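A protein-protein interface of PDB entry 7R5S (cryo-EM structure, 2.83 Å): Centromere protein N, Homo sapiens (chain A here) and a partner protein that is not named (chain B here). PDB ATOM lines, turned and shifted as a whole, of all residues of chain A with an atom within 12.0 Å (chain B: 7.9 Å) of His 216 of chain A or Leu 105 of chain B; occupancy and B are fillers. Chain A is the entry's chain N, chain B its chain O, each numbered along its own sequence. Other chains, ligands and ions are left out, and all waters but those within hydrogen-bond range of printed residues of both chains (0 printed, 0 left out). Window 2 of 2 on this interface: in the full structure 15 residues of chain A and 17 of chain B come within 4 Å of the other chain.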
ATOM      1  N   THR A 212       8.918  21.758   2.992  1.00  0.00           N
ATOM      2  CA  THR A 212       8.241  20.573   2.478  1.00  0.00           C
ATOM      3  C   THR A 212       7.349  20.985   1.317  1.00  0.00           C
ATOM      4  O   THR A 212       6.445  21.810   1.488  1.00  0.00           O
ATOM      5  CB  THR A 212       7.418  19.889   3.571  1.00  0.00           C
ATOM      6  OG1 THR A 212       6.604  20.859   4.239  1.00  0.00           O
ATOM      7  CG2 THR A 212       8.332  19.217   4.584  1.00  0.00           C
ATOM      8  N   PHE A 213       7.601  20.410   0.144  1.00  0.00           N
ATOM      9  CA  PHE A 213       6.851  20.727  -1.062  1.00  0.00           C
ATOM     10  C   PHE A 213       6.369  19.443  -1.719  1.00  0.00           C
ATOM     11  O   PHE A 213       7.088  18.441  -1.748  1.00  0.00           O
ATOM     12  CB  PHE A 213       7.703  21.533  -2.050  1.00  0.00           C
ATOM     13  CG  PHE A 213       8.239  22.815  -1.481  1.00  0.00           C
ATOM     14  CD1 PHE A 213       7.497  23.982  -1.549  1.00  0.00           C
ATOM     15  CD2 PHE A 213       9.485  22.854  -0.878  1.00  0.00           C
ATOM     16  CE1 PHE A 213       7.987  25.161  -1.027  1.00  0.00           C
ATOM     17  CE2 PHE A 213       9.979  24.031  -0.353  1.00  0.00           C
ATOM     18  CZ  PHE A 213       9.229  25.186  -0.427  1.00  0.00           C
ATOM     19  N   GLU A 214       5.148  19.482  -2.245  1.00  0.00           N
ATOM     20  CA  GLU A 214       4.537  18.321  -2.879  1.00  0.00           C
ATOM     21  C   GLU A 214       4.917  18.270  -4.353  1.00  0.00           C
ATOM     22  O   GLU A 214       4.735  19.251  -5.082  1.00  0.00           O
ATOM     23  CB  GLU A 214       3.016  18.360  -2.727  1.00  0.00           C
ATOM     24  CG  GLU A 214       2.508  17.901  -1.367  1.00  0.00           C
ATOM     25  CD  GLU A 214       2.816  18.890  -0.259  1.00  0.00           C
ATOM     26  OE1 GLU A 214       3.033  20.082  -0.564  1.00  0.00           O
ATOM     27  OE2 GLU A 214       2.843  18.474   0.919  1.00  0.00           O
ATOM     28  N   THR A 215       5.440  17.126  -4.787  1.00  0.00           N
ATOM     29  CA  THR A 215       5.816  16.930  -6.178  1.00  0.00           C
ATOM     30  C   THR A 215       5.847  15.438  -6.472  1.00  0.00           C
ATOM     31  O   THR A 215       6.092  14.622  -5.580  1.00  0.00           O
ATOM     32  CB  THR A 215       7.177  17.563  -6.494  1.00  0.00           C
ATOM     33  OG1 THR A 215       7.547  17.257  -7.844  1.00  0.00           O
ATOM     34  CG2 THR A 215       8.245  17.038  -5.547  1.00  0.00           C
ATOM     35  N   HIS A 216       5.588  15.092  -7.729  1.00  0.00           N
ATOM     36  CA  HIS A 216       5.624  13.706  -8.194  1.00  0.00           C
ATOM     37  C   HIS A 216       6.827  13.561  -9.123  1.00  0.00           C
ATOM     38  O   HIS A 216       6.717  13.714 -10.340  1.00  0.00           O
ATOM     39  CB  HIS A 216       4.319  13.314  -8.889  1.00  0.00           C
ATOM     40  CG  HIS A 216       3.740  14.390  -9.754  1.00  0.00           C
ATOM     41  ND1 HIS A 216       2.773  15.263  -9.309  1.00  0.00           N
ATOM     42  CD2 HIS A 216       3.985  14.725 -11.043  1.00  0.00           C
ATOM     43  CE1 HIS A 216       2.450  16.095 -10.283  1.00  0.00           C
ATOM     44  NE2 HIS A 216       3.172  15.790 -11.346  1.00  0.00           N
ATOM     45  N   ASN A 217       7.981  13.260  -8.536  1.00  0.00           N
ATOM     46  CA  ASN A 217       9.212  13.090  -9.299  1.00  0.00           C
ATOM     47  C   ASN A 217      10.222  12.258  -8.517  1.00  0.00           C
ATOM     48  O   ASN A 217      10.003  11.940  -7.349  1.00  0.00           O
ATOM     49  CB  ASN A 217       9.814  14.449  -9.660  1.00  0.00           C
ATOM     50  N   LEU B  98      -2.742   4.347 -16.221  1.00  0.00           N
ATOM     51  CA  LEU B  98      -2.113   4.962 -15.057  1.00  0.00           C
ATOM     52  C   LEU B  98      -0.613   5.137 -15.270  1.00  0.00           C
ATOM     53  O   LEU B  98      -0.067   6.227 -15.060  1.00  0.00           O
ATOM     54  CB  LEU B  98      -2.387   4.122 -13.808  1.00  0.00           C
ATOM     55  CG  LEU B  98      -3.729   4.358 -13.114  1.00  0.00           C
ATOM     56  CD1 LEU B  98      -3.910   3.394 -11.953  1.00  0.00           C
ATOM     57  CD2 LEU B  98      -3.835   5.797 -12.636  1.00  0.00           C
ATOM     58  N   GLU B  99       0.074   4.069 -15.684  1.00  0.00           N
ATOM     59  CA  GLU B  99       1.510   4.184 -15.919  1.00  0.00           C
ATOM     60  C   GLU B  99       1.811   5.123 -17.080  1.00  0.00           C
ATOM     61  O   GLU B  99       2.835   5.816 -17.061  1.00  0.00           O
ATOM     62  CB  GLU B  99       2.128   2.803 -16.155  1.00  0.00           C
ATOM     63  CG  GLU B  99       1.620   2.063 -17.379  1.00  0.00           C
ATOM     64  CD  GLU B  99       2.448   2.336 -18.620  1.00  0.00           C
ATOM     65  OE1 GLU B  99       3.542   2.924 -18.490  1.00  0.00           O
ATOM     66  OE2 GLU B  99       2.004   1.962 -19.726  1.00  0.00           O
ATOM     67  N   ASN B 100       0.920   5.194 -18.074  1.00  0.00           N
ATOM     68  CA  ASN B 100       1.125   6.110 -19.190  1.00  0.00           C
ATOM     69  C   ASN B 100       1.076   7.559 -18.726  1.00  0.00           C
ATOM     70  O   ASN B 100       1.960   8.358 -19.057  1.00  0.00           O
ATOM     71  CB  ASN B 100       0.078   5.852 -20.275  1.00  0.00           C
ATOM     72  CG  ASN B 100       0.276   6.729 -21.494  1.00  0.00           C
ATOM     73  OD1 ASN B 100       1.389   7.166 -21.786  1.00  0.00           O
ATOM     74  ND2 ASN B 100      -0.808   6.992 -22.215  1.00  0.00           N
ATOM     75  N   VAL B 101       0.050   7.919 -17.950  1.00  0.00           N
ATOM     76  CA  VAL B 101      -0.044   9.303 -17.491  1.00  0.00           C
ATOM     77  C   VAL B 101       1.059   9.616 -16.485  1.00  0.00           C
ATOM     78  O   VAL B 101       1.553  10.750 -16.431  1.00  0.00           O
ATOM     79  CB  VAL B 101      -1.445   9.604 -16.923  1.00  0.00           C
ATOM     80  CG1 VAL B 101      -2.509   9.364 -17.984  1.00  0.00           C
ATOM     81  CG2 VAL B 101      -1.726   8.779 -15.682  1.00  0.00           C
ATOM     82  N   LYS B 102       1.495   8.625 -15.700  1.00  0.00           N
ATOM     83  CA  LYS B 102       2.611   8.858 -14.788  1.00  0.00           C
ATOM     84  C   LYS B 102       3.899   9.136 -15.554  1.00  0.00           C
ATOM     85  O   LYS B 102       4.649  10.057 -15.206  1.00  0.00           O
ATOM     86  CB  LYS B 102       2.787   7.662 -13.854  1.00  0.00           C
ATOM     87  CG  LYS B 102       1.728   7.563 -12.768  1.00  0.00           C
ATOM     88  CD  LYS B 102       1.970   6.364 -11.868  1.00  0.00           C
ATOM     89  CE  LYS B 102       0.860   6.213 -10.840  1.00  0.00           C
ATOM     90  NZ  LYS B 102      -0.462   5.986 -11.485  1.00  0.00           N
ATOM     91  N   ALA B 103       4.176   8.350 -16.600  1.00  0.00           N
ATOM     92  CA  ALA B 103       5.350   8.608 -17.425  1.00  0.00           C
ATOM     93  C   ALA B 103       5.243   9.953 -18.130  1.00  0.00           C
ATOM     94  O   ALA B 103       6.245  10.661 -18.289  1.00  0.00           O
ATOM     95  CB  ALA B 103       5.534   7.480 -18.442  1.00  0.00           C
ATOM     96  N   ILE B 104       4.033  10.327 -18.554  1.00  0.00           N
ATOM     97  CA  ILE B 104       3.843  11.617 -19.210  1.00  0.00           C
ATOM     98  C   ILE B 104       4.157  12.757 -18.250  1.00  0.00           C
ATOM     99  O   ILE B 104       4.806  13.740 -18.622  1.00  0.00           O
ATOM    100  CB  ILE B 104       2.416  11.724 -19.778  1.00  0.00           C
ATOM    101  CG1 ILE B 104       2.296  10.907 -21.066  1.00  0.00           C
ATOM    102  CG2 ILE B 104       2.046  13.176 -20.037  1.00  0.00           C
ATOM    103  CD1 ILE B 104       0.932  10.986 -21.716  1.00  0.00           C
ATOM    104  N   LEU B 105       3.719  12.638 -16.993  1.00  0.00           N
ATOM    105  CA  LEU B 105       4.031  13.673 -16.009  1.00  0.00           C
ATOM    106  C   LEU B 105       5.525  13.709 -15.694  1.00  0.00           C
ATOM    107  O   LEU B 105       6.117  14.792 -15.571  1.00  0.00           O
ATOM    108  CB  LEU B 105       3.218  13.448 -14.735  1.00  0.00           C
ATOM    109  CG  LEU B 105       1.937  14.272 -14.578  1.00  0.00           C
ATOM    110  CD1 LEU B 105       1.036  14.126 -15.795  1.00  0.00           C
ATOM    111  CD2 LEU B 105       1.195  13.873 -13.313  1.00  0.00           C
ATOM    112  N   GLN B 106       6.152  12.537 -15.565  1.00  0.00           N
ATOM    113  CA  GLN B 106       7.587  12.497 -15.300  1.00  0.00           C
ATOM    114  C   GLN B 106       8.386  13.109 -16.444  1.00  0.00           C
ATOM    115  O   GLN B 106       9.436  13.716 -16.211  1.00  0.00           O
ATOM    116  CB  GLN B 106       8.035  11.058 -15.046  1.00  0.00           C
ATOM    117  CG  GLN B 106       8.023  10.649 -13.580  1.00  0.00           C
ATOM    118  CD  GLN B 106       6.642  10.728 -12.960  1.00  0.00           C
ATOM    119  OE1 GLN B 106       6.254  11.756 -12.406  1.00  0.00           O
ATOM    120  NE2 GLN B 106       5.891   9.637 -13.051  1.00  0.00           N
ATOM    121  N   ALA B 107       7.908  12.961 -17.681  1.00  0.00           N
ATOM    122  CA  ALA B 107       8.582  13.584 -18.815  1.00  0.00           C
ATOM    123  C   ALA B 107       8.290  15.078 -18.886  1.00  0.00           C
ATOM    124  O   ALA B 107       9.152  15.861 -19.297  1.00  0.00           O
ATOM    125  CB  ALA B 107       8.168  12.895 -20.114  1.00  0.00           C
ATOM    126  N   TYR B 108       7.078  15.484 -18.499  1.00  0.00           N
ATOM    127  CA  TYR B 108       6.757  16.905 -18.420  1.00  0.00           C
ATOM    128  C   TYR B 108       7.629  17.609 -17.393  1.00  0.00           C
ATOM    129  O   TYR B 108       7.901  18.807 -17.524  1.00  0.00           O
ATOM    130  CB  TYR B 108       5.280  17.086 -18.069  1.00  0.00           C
ATOM    131  CG  TYR B 108       4.668  18.352 -18.615  1.00  0.00           C
ATOM    132  CD1 TYR B 108       3.942  18.337 -19.796  1.00  0.00           C
ATOM    133  CD2 TYR B 108       4.815  19.562 -17.952  1.00  0.00           C
ATOM    134  CE1 TYR B 108       3.378  19.487 -20.301  1.00  0.00           C
ATOM    135  CE2 TYR B 108       4.256  20.721 -18.451  1.00  0.00           C
ATOM    136  CZ  TYR B 108       3.538  20.676 -19.628  1.00  0.00           C
ATOM    137  OH  TYR B 108       2.975  21.824 -20.134  1.00  0.00           O
ATOM    138  N   HIS B 109       8.060  16.883 -16.360  1.00  0.00           N
ATOM    139  CA  HIS B 109       8.993  17.453 -15.393  1.00  0.00           C
ATOM    140  C   HIS B 109      10.291  17.910 -16.055  1.00  0.00           C
ATOM    141  O   HIS B 109      10.967  18.809 -15.540  1.00  0.00           O
ATOM    142  CB  HIS B 109       9.286  16.434 -14.290  1.00  0.00           C
ATOM    143  CG  HIS B 109      10.465  16.786 -13.437  1.00  0.00           C
ATOM    144  ND1 HIS B 109      11.742  16.347 -13.714  1.00  0.00           N
ATOM    145  CD2 HIS B 109      10.560  17.536 -12.313  1.00  0.00           C
ATOM    146  CE1 HIS B 109      12.573  16.811 -12.798  1.00  0.00           C
ATOM    147  NE2 HIS B 109      11.882  17.534 -11.936  1.00  0.00           N
ATOM    148  N   PHE B 110      10.648  17.318 -17.197  1.00  0.00           N
ATOM    149  CA  PHE B 110      11.908  17.614 -17.868  1.00  0.00           C
ATOM    150  C   PHE B 110      11.888  18.912 -18.667  1.00  0.00           C
ATOM    151  O   PHE B 110      12.950  19.351 -19.120  1.00  0.00           O
ATOM    152  CB  PHE B 110      12.286  16.461 -18.803  1.00  0.00           C
ATOM    153  CG  PHE B 110      13.257  15.485 -18.206  1.00  0.00           C
ATOM    154  CD1 PHE B 110      12.824  14.503 -17.331  1.00  0.00           C
ATOM    155  CD2 PHE B 110      14.603  15.542 -18.527  1.00  0.00           C
ATOM    156  CE1 PHE B 110      13.715  13.601 -16.783  1.00  0.00           C
ATOM    157  CE2 PHE B 110      15.499  14.644 -17.982  1.00  0.00           C
ATOM    158  CZ  PHE B 110      15.055  13.672 -17.109  1.00  0.00           C
ATOM    159  N   THR B 111      10.722  19.533 -18.857  1.00  0.00           N
ATOM    160  CA  THR B 111      10.636  20.705 -19.722  1.00  0.00           C
ATOM    161  C   THR B 111      11.256  21.951 -19.103  1.00  0.00           C
ATOM    162  O   THR B 111      11.473  22.933 -19.822  1.00  0.00           O
ATOM    163  CB  THR B 111       9.179  20.991 -20.089  1.00  0.00           C
ATOM    164  OG1 THR B 111       9.136  21.884 -21.208  1.00  0.00           O
ATOM    165  CG2 THR B 111       8.449  21.632 -18.920  1.00  0.00           C
ATOM    166  N   LEU B 113       9.999  23.492 -16.067  1.00  0.00           N
ATOM    167  CA  LEU B 113       9.110  23.867 -14.978  1.00  0.00           C
ATOM    168  C   LEU B 113       7.964  22.869 -14.906  1.00  0.00           C
ATOM    169  O   LEU B 113       7.386  22.498 -15.931  1.00  0.00           O
ATOM    170  CB  LEU B 113       8.566  25.295 -15.148  1.00  0.00           C
ATOM    171  CG  LEU B 113       7.641  25.630 -16.322  1.00  0.00           C
ATOM    172  CD1 LEU B 113       6.787  26.842 -15.988  1.00  0.00           C
ATOM    173  CD2 LEU B 113       8.434  25.880 -17.596  1.00  0.00           C
ATOM    174  N   SER B 114       7.652  22.430 -13.690  1.00  0.00           N
ATOM    175  CA  SER B 114       6.592  21.460 -13.457  1.00  0.00           C
ATOM    176  C   SER B 114       5.649  21.991 -12.387  1.00  0.00           C
ATOM    177  O   SER B 114       5.953  22.958 -11.687  1.00  0.00           O
ATOM    178  CB  SER B 114       7.161  20.097 -13.041  1.00  0.00           C
ATOM    179  OG  SER B 114       7.358  20.034 -11.639  1.00  0.00           O
ATOM    180  N   GLY B 115       4.499  21.346 -12.258  1.00  0.00           N
ATOM    181  CA  GLY B 115       3.507  21.774 -11.286  1.00  0.00           C
ATOM    182  C   GLY B 115       2.683  20.610 -10.790  1.00  0.00           C
ATOM    183  O   GLY B 115       2.460  19.630 -11.508  1.00  0.00           O
ATOM    184  N   LYS B 116       2.228  20.721  -9.543  1.00  0.00           N
ATOM    185  CA  LYS B 116       1.384  19.702  -8.933  1.00  0.00           C
ATOM    186  C   LYS B 116       0.255  20.367  -8.161  1.00  0.00           C
ATOM    187  O   LYS B 116       0.476  21.343  -7.438  1.00  0.00           O
ATOM    188  CB  LYS B 116       2.185  18.789  -7.993  1.00  0.00           C
ATOM    189  CG  LYS B 116       1.347  17.697  -7.345  1.00  0.00           C
ATOM    190  CD  LYS B 116       2.167  16.849  -6.390  1.00  0.00           C
ATOM    191  CE  LYS B 116       1.317  15.760  -5.757  1.00  0.00           C
ATOM    192  NZ  LYS B 116       2.105  14.910  -4.824  1.00  0.00           N
ATOM    193  N   LEU B 117      -0.952  19.828  -8.310  1.00  0.00           N
ATOM    194  CA  LEU B 117      -2.113  20.352  -7.604  1.00  0.00           C
ATOM    195  C   LEU B 117      -2.123  19.857  -6.163  1.00  0.00           C
ATOM    196  O   LEU B 117      -2.035  18.651  -5.911  1.00  0.00           O
ATOM    197  CB  LEU B 117      -3.400  19.936  -8.314  1.00  0.00           C
ATOM    198  CG  LEU B 117      -3.731  20.668  -9.615  1.00  0.00           C
ATOM    199  CD1 LEU B 117      -4.913  20.014 -10.311  1.00  0.00           C
ATOM    200  CD2 LEU B 117      -4.016  22.134  -9.340  1.00  0.00           C
ATOM    201  N   CYS B 123       1.641  23.867  -6.659  1.00  0.00           N
ATOM    202  CA  CYS B 123       3.038  23.981  -6.262  1.00  0.00           C
ATOM    203  C   CYS B 123       3.893  23.809  -7.508  1.00  0.00           C
ATOM    204  O   CYS B 123       3.788  22.789  -8.198  1.00  0.00           O
ATOM    205  CB  CYS B 123       3.400  22.936  -5.205  1.00  0.00           C
ATOM    206  SG  CYS B 123       4.835  23.361  -4.193  1.00  0.00           S
ATOM    207  N   PHE B 139      11.304  25.699  -5.483  1.00  0.00           N
ATOM    208  CA  PHE B 139       9.871  25.463  -5.389  1.00  0.00           C
ATOM    209  C   PHE B 139       9.150  26.740  -4.981  1.00  0.00           C
ATOM    210  O   PHE B 139       9.700  27.585  -4.269  1.00  0.00           O
ATOM    211  CB  PHE B 139       9.549  24.351  -4.382  1.00  0.00           C
ATOM    212  CG  PHE B 139      10.118  23.012  -4.751  1.00  0.00           C
ATOM    213  CD1 PHE B 139       9.378  22.115  -5.502  1.00  0.00           C
ATOM    214  CD2 PHE B 139      11.391  22.648  -4.345  1.00  0.00           C
ATOM    215  CE1 PHE B 139       9.896  20.882  -5.841  1.00  0.00           C
ATOM    216  CE2 PHE B 139      11.915  21.417  -4.683  1.00  0.00           C
ATOM    217  CZ  PHE B 139      11.167  20.533  -5.432  1.00  0.00           C
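The backbone carbonyl oxygen (O) of His 216 of chain A sits close to the side-chain amide oxygen (OE1) of Gln 106 of chain B (2.9 Å).
The backbone carbonyl oxygen (O) of Lys 116 of chain B lies within hydrogen-bond range of the backbone NH (N) of Cys 123 of chain B (2.9 Å).
The backbone carbonyl oxygen (O) of Lys 102 of chain B lies within hydrogen-bond range of the side-chain amide nitrogen (NE2) of Gln 106 of chain B (2.5 Å).
Among the printed residues, pairs that only touch across the chains: Phe 213 of chain A with Cys 123 of chain B (3.8 Å), Phe 213 of chain A with Phe 139 of chain B (3.5 Å), Glu 214 of chain A with Lys 116 of chain B (3.7 Å), Glu 214 of chain A with Cys 123 of chain B (3.9 Å), Thr 215 of chain A with Lys 116 of chain B (3.7 Å), His 216 of chain A with Leu 105 of chain B (3.4 Å), His 216 of chain A with Gly 115 of chain B (3.7 Å) and His 216 of chain A with Lys 116 of chain B (3.4 Å).
Of the printed residues of chain B, Phe 213 of chain A touches Cys 123 (3.8 Å) and Phe 139 (3.5 Å).
Of the printed residues of chain B, Glu 214 of chain A touches Lys 116 and Cys 123.
Printed residues of chain B within 4 Å of Thr 215 of chain A: Lys 116 (3.7 Å).
Of chain B, only Leu 105, Gln 106, Gly 115 and Lys 116 come within 4 Å of His 216 of chain A.
No residue of chain A comes within 4 Å of Val 101 of chain B.
No residue of chain A comes within 4 Å of Ala 103 of chain B.
No residue of chain A comes within 4 Å of Ile 104 of chain B.
Of chain A, only His 216 (3.4 Å) comes within 4 Å of Leu 105 of chain B.
Of the printed residues of chain A, Gln 106 of chain B touches His 216.
No residue of chain A comes within 4 Å of His 109 of chain B.
Leu 113 of chain B touches none of the printed residues of chain A.
Gly 115 of chain B touches one residue of chain A.
Lys 116 of chain B touches three residues of chain A.
Leu 117 of chain B touches none of the printed residues of chain A.
Printed residues of chain A within 4 Å of Cys 123 of chain B: Phe 213 and Glu 214.
Printed residues of chain A within 4 Å of Phe 139 of chain B: Phe 213 (3.5 Å).
The nearest printed residue of chain B that does not touch His 216 of chain A is Leu 117 of chain B (5.4 Å).
The nearest residue of chain A that does not touch Leu 105 of chain B is Asn 217 of chain A (7.0 Å).
The nearest printed residue of chain B that does not touch Phe 213 of chain A is Lys 116 of chain B (6.8 Å).
Of the 6 printed residues of chain A, 4 touch a printed residue of chain B.
Of the 21 printed residues of chain B, 6 touch a printed residue of chain A.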
